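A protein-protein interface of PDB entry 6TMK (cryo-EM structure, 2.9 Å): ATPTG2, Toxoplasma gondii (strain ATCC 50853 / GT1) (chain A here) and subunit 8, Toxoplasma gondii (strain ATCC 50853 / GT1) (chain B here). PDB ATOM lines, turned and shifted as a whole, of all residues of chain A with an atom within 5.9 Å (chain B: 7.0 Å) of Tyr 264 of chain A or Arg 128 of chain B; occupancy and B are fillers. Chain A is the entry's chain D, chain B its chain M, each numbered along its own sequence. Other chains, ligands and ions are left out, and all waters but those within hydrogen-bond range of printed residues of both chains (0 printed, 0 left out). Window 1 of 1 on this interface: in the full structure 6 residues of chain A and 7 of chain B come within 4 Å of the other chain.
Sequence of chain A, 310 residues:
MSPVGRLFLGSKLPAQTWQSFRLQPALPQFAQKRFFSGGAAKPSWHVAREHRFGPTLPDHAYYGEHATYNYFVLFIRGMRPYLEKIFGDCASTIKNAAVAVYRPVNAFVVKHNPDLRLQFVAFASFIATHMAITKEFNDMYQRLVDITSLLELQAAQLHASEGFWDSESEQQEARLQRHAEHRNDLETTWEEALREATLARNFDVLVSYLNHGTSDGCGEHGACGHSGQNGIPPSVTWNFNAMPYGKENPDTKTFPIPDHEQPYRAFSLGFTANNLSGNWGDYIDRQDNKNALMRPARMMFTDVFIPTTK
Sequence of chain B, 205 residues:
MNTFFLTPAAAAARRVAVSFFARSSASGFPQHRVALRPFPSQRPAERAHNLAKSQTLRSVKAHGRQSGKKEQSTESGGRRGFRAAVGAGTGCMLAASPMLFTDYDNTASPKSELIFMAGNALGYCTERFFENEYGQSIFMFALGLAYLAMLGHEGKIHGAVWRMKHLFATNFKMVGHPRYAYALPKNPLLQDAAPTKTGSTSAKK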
ATOM      1  N   ASP A 259      18.708   2.545  -7.775  1.00  0.00           N
ATOM      2  CA  ASP A 259      19.039   3.470  -8.842  1.00  0.00           C
ATOM      3  C   ASP A 259      19.812   4.656  -8.298  1.00  0.00           C
ATOM      4  O   ASP A 259      20.686   5.194  -8.984  1.00  0.00           O
ATOM      5  CB  ASP A 259      17.763   3.929  -9.542  1.00  0.00           C
ATOM      6  CG  ASP A 259      17.309   2.965 -10.625  1.00  0.00           C
ATOM      7  OD1 ASP A 259      18.032   1.986 -10.904  1.00  0.00           O
ATOM      8  OD2 ASP A 259      16.217   3.181 -11.194  1.00  0.00           O
ATOM      9  N   GLN A 262      23.366   3.660  -8.320  1.00  0.00           N
ATOM     10  CA  GLN A 262      24.062   3.272  -9.537  1.00  0.00           C
ATOM     11  C   GLN A 262      24.708   4.497 -10.186  1.00  0.00           C
ATOM     12  O   GLN A 262      24.161   5.601 -10.120  1.00  0.00           O
ATOM     13  CB  GLN A 262      23.106   2.610 -10.520  1.00  0.00           C
ATOM     14  CG  GLN A 262      22.595   1.277 -10.052  1.00  0.00           C
ATOM     15  CD  GLN A 262      22.246   0.366 -11.192  1.00  0.00           C
ATOM     16  OE1 GLN A 262      21.132   0.399 -11.714  1.00  0.00           O
ATOM     17  NE2 GLN A 262      23.208  -0.438 -11.610  1.00  0.00           N
ATOM     18  N   PRO A 263      25.868   4.359 -10.824  1.00  0.00           N
ATOM     19  CA  PRO A 263      26.549   5.524 -11.389  1.00  0.00           C
ATOM     20  C   PRO A 263      26.075   5.893 -12.789  1.00  0.00           C
ATOM     21  O   PRO A 263      25.530   5.080 -13.534  1.00  0.00           O
ATOM     22  CB  PRO A 263      28.014   5.074 -11.408  1.00  0.00           C
ATOM     23  CG  PRO A 263      27.938   3.649 -11.648  1.00  0.00           C
ATOM     24  CD  PRO A 263      26.692   3.148 -10.963  1.00  0.00           C
ATOM     25  N   TYR A 264      26.318   7.152 -13.137  1.00  0.00           N
ATOM     26  CA  TYR A 264      25.879   7.690 -14.414  1.00  0.00           C
ATOM     27  C   TYR A 264      26.972   7.606 -15.465  1.00  0.00           C
ATOM     28  O   TYR A 264      28.163   7.734 -15.173  1.00  0.00           O
ATOM     29  CB  TYR A 264      25.479   9.158 -14.281  1.00  0.00           C
ATOM     30  CG  TYR A 264      24.204   9.438 -13.535  1.00  0.00           C
ATOM     31  CD1 TYR A 264      23.049   8.728 -13.790  1.00  0.00           C
ATOM     32  CD2 TYR A 264      24.157  10.444 -12.589  1.00  0.00           C
ATOM     33  CE1 TYR A 264      21.891   8.996 -13.109  1.00  0.00           C
ATOM     34  CE2 TYR A 264      23.007  10.722 -11.906  1.00  0.00           C
ATOM     35  CZ  TYR A 264      21.872   9.997 -12.169  1.00  0.00           C
ATOM     36  OH  TYR A 264      20.716  10.272 -11.485  1.00  0.00           O
ATOM     37  N   ARG A 265      26.544   7.399 -16.702  1.00  0.00           N
ATOM     38  CA  ARG A 265      27.434   7.473 -17.845  1.00  0.00           C
ATOM     39  C   ARG A 265      27.630   8.921 -18.272  1.00  0.00           C
ATOM     40  O   ARG A 265      26.740   9.764 -18.124  1.00  0.00           O
ATOM     41  CB  ARG A 265      26.872   6.659 -19.003  1.00  0.00           C
ATOM     42  CG  ARG A 265      27.784   6.516 -20.172  1.00  0.00           C
ATOM     43  CD  ARG A 265      27.176   5.620 -21.201  1.00  0.00           C
ATOM     44  NE  ARG A 265      27.949   5.579 -22.430  1.00  0.00           N
ATOM     45  CZ  ARG A 265      27.716   6.330 -23.498  1.00  0.00           C
ATOM     46  NH1 ARG A 265      26.727   7.205 -23.512  1.00  0.00           N
ATOM     47  NH2 ARG A 265      28.486   6.206 -24.557  1.00  0.00           N
ATOM     48  N   ALA A 266      28.806   9.206 -18.810  1.00  0.00           N
ATOM     49  CA  ALA A 266      29.134  10.567 -19.202  1.00  0.00           C
ATOM     50  C   ALA A 266      28.248  11.025 -20.350  1.00  0.00           C
ATOM     51  O   ALA A 266      27.810  10.229 -21.185  1.00  0.00           O
ATOM     52  CB  ALA A 266      30.598  10.682 -19.600  1.00  0.00           C
ATOM     53  N   PHE A 267      27.981  12.325 -20.384  1.00  0.00           N
ATOM     54  CA  PHE A 267      27.119  12.923 -21.388  1.00  0.00           C
ATOM     55  C   PHE A 267      27.904  13.931 -22.209  1.00  0.00           C
ATOM     56  O   PHE A 267      28.558  14.820 -21.654  1.00  0.00           O
ATOM     57  CB  PHE A 267      25.917  13.604 -20.745  1.00  0.00           C
ATOM     58  CG  PHE A 267      24.838  13.941 -21.713  1.00  0.00           C
ATOM     59  CD1 PHE A 267      23.981  12.967 -22.171  1.00  0.00           C
ATOM     60  CD2 PHE A 267      24.686  15.231 -22.175  1.00  0.00           C
ATOM     61  CE1 PHE A 267      22.993  13.272 -23.064  1.00  0.00           C
ATOM     62  CE2 PHE A 267      23.700  15.540 -23.067  1.00  0.00           C
ATOM     63  CZ  PHE A 267      22.850  14.560 -23.514  1.00  0.00           C
ATOM     64  N   LEU B 122      15.095  18.404 -11.604  1.00  0.00           N
ATOM     65  CA  LEU B 122      16.230  19.313 -11.493  1.00  0.00           C
ATOM     66  C   LEU B 122      17.403  18.645 -10.793  1.00  0.00           C
ATOM     67  O   LEU B 122      18.559  18.894 -11.139  1.00  0.00           O
ATOM     68  CB  LEU B 122      15.824  20.581 -10.752  1.00  0.00           C
ATOM     69  CG  LEU B 122      15.258  21.755 -11.549  1.00  0.00           C
ATOM     70  CD1 LEU B 122      16.243  22.280 -12.571  1.00  0.00           C
ATOM     71  CD2 LEU B 122      13.974  21.362 -12.220  1.00  0.00           C
ATOM     72  N   GLY B 123      17.126  17.785  -9.815  1.00  0.00           N
ATOM     73  CA  GLY B 123      18.197  17.063  -9.153  1.00  0.00           C
ATOM     74  C   GLY B 123      18.879  16.075 -10.075  1.00  0.00           C
ATOM     75  O   GLY B 123      20.103  15.920 -10.046  1.00  0.00           O
ATOM     76  N   TYR B 124      18.096  15.392 -10.907  1.00  0.00           N
ATOM     77  CA  TYR B 124      18.661  14.490 -11.898  1.00  0.00           C
ATOM     78  C   TYR B 124      19.545  15.254 -12.872  1.00  0.00           C
ATOM     79  O   TYR B 124      20.681  14.849 -13.147  1.00  0.00           O
ATOM     80  CB  TYR B 124      17.538  13.766 -12.640  1.00  0.00           C
ATOM     81  CG  TYR B 124      18.028  12.910 -13.776  1.00  0.00           C
ATOM     82  CD1 TYR B 124      18.589  11.676 -13.533  1.00  0.00           C
ATOM     83  CD2 TYR B 124      17.941  13.338 -15.087  1.00  0.00           C
ATOM     84  CE1 TYR B 124      19.043  10.892 -14.552  1.00  0.00           C
ATOM     85  CE2 TYR B 124      18.395  12.560 -16.115  1.00  0.00           C
ATOM     86  CZ  TYR B 124      18.949  11.334 -15.842  1.00  0.00           C
ATOM     87  OH  TYR B 124      19.408  10.540 -16.863  1.00  0.00           O
ATOM     88  N   CYS B 125      19.037  16.363 -13.411  1.00  0.00           N
ATOM     89  CA  CYS B 125      19.830  17.132 -14.360  1.00  0.00           C
ATOM     90  C   CYS B 125      21.034  17.780 -13.692  1.00  0.00           C
ATOM     91  O   CYS B 125      22.037  18.042 -14.358  1.00  0.00           O
ATOM     92  CB  CYS B 125      18.969  18.191 -15.049  1.00  0.00           C
ATOM     93  SG  CYS B 125      17.481  17.580 -15.853  1.00  0.00           S
ATOM     94  N   THR B 126      20.968  18.039 -12.389  1.00  0.00           N
ATOM     95  CA  THR B 126      22.135  18.561 -11.692  1.00  0.00           C
ATOM     96  C   THR B 126      23.202  17.487 -11.550  1.00  0.00           C
ATOM     97  O   THR B 126      24.369  17.708 -11.891  1.00  0.00           O
ATOM     98  CB  THR B 126      21.739  19.100 -10.317  1.00  0.00           C
ATOM     99  OG1 THR B 126      20.808  20.174 -10.465  1.00  0.00           O
ATOM    100  CG2 THR B 126      22.954  19.593  -9.572  1.00  0.00           C
ATOM    101  N   GLU B 127      22.819  16.312 -11.050  1.00  0.00           N
ATOM    102  CA  GLU B 127      23.790  15.245 -10.866  1.00  0.00           C
ATOM    103  C   GLU B 127      24.351  14.756 -12.194  1.00  0.00           C
ATOM    104  O   GLU B 127      25.480  14.257 -12.239  1.00  0.00           O
ATOM    105  CB  GLU B 127      23.155  14.091 -10.095  1.00  0.00           C
ATOM    106  CG  GLU B 127      22.894  14.390  -8.638  1.00  0.00           C
ATOM    107  CD  GLU B 127      22.398  13.178  -7.873  1.00  0.00           C
ATOM    108  OE1 GLU B 127      21.274  13.234  -7.331  1.00  0.00           O
ATOM    109  OE2 GLU B 127      23.129  12.168  -7.811  1.00  0.00           O
ATOM    110  N   ARG B 128      23.592  14.890 -13.282  1.00  0.00           N
ATOM    111  CA  ARG B 128      24.017  14.366 -14.571  1.00  0.00           C
ATOM    112  C   ARG B 128      24.738  15.395 -15.436  1.00  0.00           C
ATOM    113  O   ARG B 128      25.716  15.051 -16.107  1.00  0.00           O
ATOM    114  CB  ARG B 128      22.808  13.819 -15.328  1.00  0.00           C
ATOM    115  CG  ARG B 128      23.152  13.047 -16.576  1.00  0.00           C
ATOM    116  CD  ARG B 128      23.125  11.567 -16.371  1.00  0.00           C
ATOM    117  NE  ARG B 128      23.888  10.869 -17.399  1.00  0.00           N
ATOM    118  CZ  ARG B 128      23.381  10.430 -18.546  1.00  0.00           C
ATOM    119  NH1 ARG B 128      22.103  10.614 -18.835  1.00  0.00           N
ATOM    120  NH2 ARG B 128      24.161   9.804 -19.412  1.00  0.00           N
ATOM    121  N   PHE B 129      24.288  16.649 -15.444  1.00  0.00           N
ATOM    122  CA  PHE B 129      24.785  17.646 -16.381  1.00  0.00           C
ATOM    123  C   PHE B 129      25.460  18.826 -15.704  1.00  0.00           C
ATOM    124  O   PHE B 129      26.601  19.155 -16.044  1.00  0.00           O
ATOM    125  CB  PHE B 129      23.631  18.155 -17.256  1.00  0.00           C
ATOM    126  CG  PHE B 129      22.805  17.070 -17.869  1.00  0.00           C
ATOM    127  CD1 PHE B 129      23.368  16.161 -18.735  1.00  0.00           C
ATOM    128  CD2 PHE B 129      21.465  16.956 -17.574  1.00  0.00           C
ATOM    129  CE1 PHE B 129      22.609  15.167 -19.295  1.00  0.00           C
ATOM    130  CE2 PHE B 129      20.706  15.962 -18.130  1.00  0.00           C
ATOM    131  CZ  PHE B 129      21.281  15.065 -18.994  1.00  0.00           C
ATOM    132  N   PHE B 130      24.790  19.478 -14.751  1.00  0.00           N
ATOM    133  CA  PHE B 130      25.183  20.829 -14.368  1.00  0.00           C
ATOM    134  C   PHE B 130      26.436  20.880 -13.509  1.00  0.00           C
ATOM    135  O   PHE B 130      27.220  21.824 -13.633  1.00  0.00           O
ATOM    136  CB  PHE B 130      24.057  21.529 -13.609  1.00  0.00           C
ATOM    137  CG  PHE B 130      22.773  21.634 -14.362  1.00  0.00           C
ATOM    138  CD1 PHE B 130      22.752  21.651 -15.737  1.00  0.00           C
ATOM    139  CD2 PHE B 130      21.580  21.728 -13.682  1.00  0.00           C
ATOM    140  CE1 PHE B 130      21.566  21.754 -16.415  1.00  0.00           C
ATOM    141  CE2 PHE B 130      20.397  21.827 -14.356  1.00  0.00           C
ATOM    142  CZ  PHE B 130      20.390  21.841 -15.724  1.00  0.00           C
ATOM    143  N   GLU B 131      26.660  19.889 -12.649  1.00  0.00           N
ATOM    144  CA  GLU B 131      27.795  19.923 -11.735  1.00  0.00           C
ATOM    145  C   GLU B 131      29.045  19.306 -12.331  1.00  0.00           C
ATOM    146  O   GLU B 131      29.917  18.838 -11.590  1.00  0.00           O
ATOM    147  CB  GLU B 131      27.433  19.263 -10.405  1.00  0.00           C
ATOM    148  CG  GLU B 131      27.270  17.771 -10.409  1.00  0.00           C
ATOM    149  CD  GLU B 131      26.708  17.254  -9.103  1.00  0.00           C
ATOM    150  OE1 GLU B 131      26.328  18.079  -8.249  1.00  0.00           O
ATOM    151  OE2 GLU B 131      26.659  16.019  -8.920  1.00  0.00           O
ATOM    152  N   ASN B 132      29.164  19.306 -13.656  1.00  0.00           N
ATOM    153  CA  ASN B 132      30.301  18.719 -14.340  1.00  0.00           C
ATOM    154  C   ASN B 132      30.665  19.597 -15.539  1.00  0.00           C
ATOM    155  O   ASN B 132      30.212  20.741 -15.671  1.00  0.00           O
ATOM    156  CB  ASN B 132      29.981  17.269 -14.721  1.00  0.00           C
ATOM    157  CG  ASN B 132      29.500  16.451 -13.531  1.00  0.00           C
ATOM    158  OD1 ASN B 132      28.357  15.988 -13.499  1.00  0.00           O
ATOM    159  ND2 ASN B 132      30.365  16.285 -12.538  1.00  0.00           N
ATOM    160  N   TYR B 134      29.932  19.432 -18.731  1.00  0.00           N
ATOM    161  CA  TYR B 134      28.819  19.850 -19.569  1.00  0.00           C
ATOM    162  C   TYR B 134      28.061  21.002 -18.927  1.00  0.00           C
ATOM    163  O   TYR B 134      27.552  21.887 -19.624  1.00  0.00           O
ATOM    164  CB  TYR B 134      27.895  18.674 -19.847  1.00  0.00           C
ATOM    165  CG  TYR B 134      27.046  18.861 -21.072  1.00  0.00           C
ATOM    166  CD1 TYR B 134      27.604  18.804 -22.336  1.00  0.00           C
ATOM    167  CD2 TYR B 134      25.691  19.099 -20.969  1.00  0.00           C
ATOM    168  CE1 TYR B 134      26.839  18.977 -23.456  1.00  0.00           C
ATOM    169  CE2 TYR B 134      24.916  19.274 -22.085  1.00  0.00           C
ATOM    170  CZ  TYR B 134      25.495  19.212 -23.328  1.00  0.00           C
ATOM    171  OH  TYR B 134      24.725  19.388 -24.450  1.00  0.00           O
ATOM    172  N   GLY B 135      28.022  21.037 -17.597  1.00  0.00           N
ATOM    173  CA  GLY B 135      27.443  22.171 -16.909  1.00  0.00           C
ATOM    174  C   GLY B 135      28.267  23.428 -17.052  1.00  0.00           C
ATOM    175  O   GLY B 135      27.718  24.530 -17.121  1.00  0.00           O
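Gln 262 of chain A touches none of the printed residues of chain B.
Printed residues of chain B within 4 Å of Arg 265 of chain A: Arg 128.
Of the printed residues of chain B, Phe 267 of chain A touches Phe 129 (3.5 Å).
Printed residues of chain A within 4 Å of Tyr 124 of chain B: Tyr 264.
Printed residues of chain A within 4 Å of Glu 127 of chain B: Tyr 264.
Of chain A, only Tyr 264 and Arg 265 come within 4 Å of Arg 128 of chain B.
Printed residues of chain A within 4 Å of Phe 129 of chain B: Phe 267 (3.5 Å).
The nearest printed residue of chain B that does not touch Phe 267 of chain A is Tyr 134 of chain B (4.05 Å).
Tyr 124 of chain B touches Tyr 264 of chain A.
Glu 127 of chain B touches Tyr 264 of chain A (CB to CE2, 3.8 Å).
Arg 128 of chain B touches Tyr 264 of chain A (CD to CG, 3.7 Å).
CG of Phe 267 of chain A touches CE1 of Phe 129 of chain B, 3.5 Å away.
Of the 13 printed residues of chain B, 4 touch a printed residue of chain A.
Printed residues of chain B that touch a printed residue of chain A: Tyr 124, Glu 127, Arg 128 and Phe 129.
Hydrophobic or aromatic side chains of chain B that line the printed part of chain A: Tyr 124 and Phe 129.
Along chain B the printed residues that touch a printed residue of chain A span positions 124 to 129.
Printed residues of chain A that touch a printed residue of chain B: Tyr 264, Arg 265 and Phe 267.
Hydrophobic or aromatic side chains of chain A within 4 Å of the printed part of chain B: Tyr 264 and Phe 267.
Among the printed residues, no Asp or Glu carboxylate lies within 4 Å of a Lys or Arg side-chain nitrogen of the other chain.
The side-chain hydroxyl (OH) of Tyr 124 of chain B is in hydrogen-bond range of the guanidinium group (NH1) of Arg 128 of chain B (3.3 Å).
The backbone NH (N) of Gly 135 of chain B lies within hydrogen-bond range of the backbone carbonyl oxygen (O) of Phe 129 of chain B (2.8 Å).
The backbone carbonyl oxygen (O) of Arg 265 of chain A is in hydrogen-bond range of the guanidinium group (NH2) of Arg 128 of chain B (2.9 Å).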
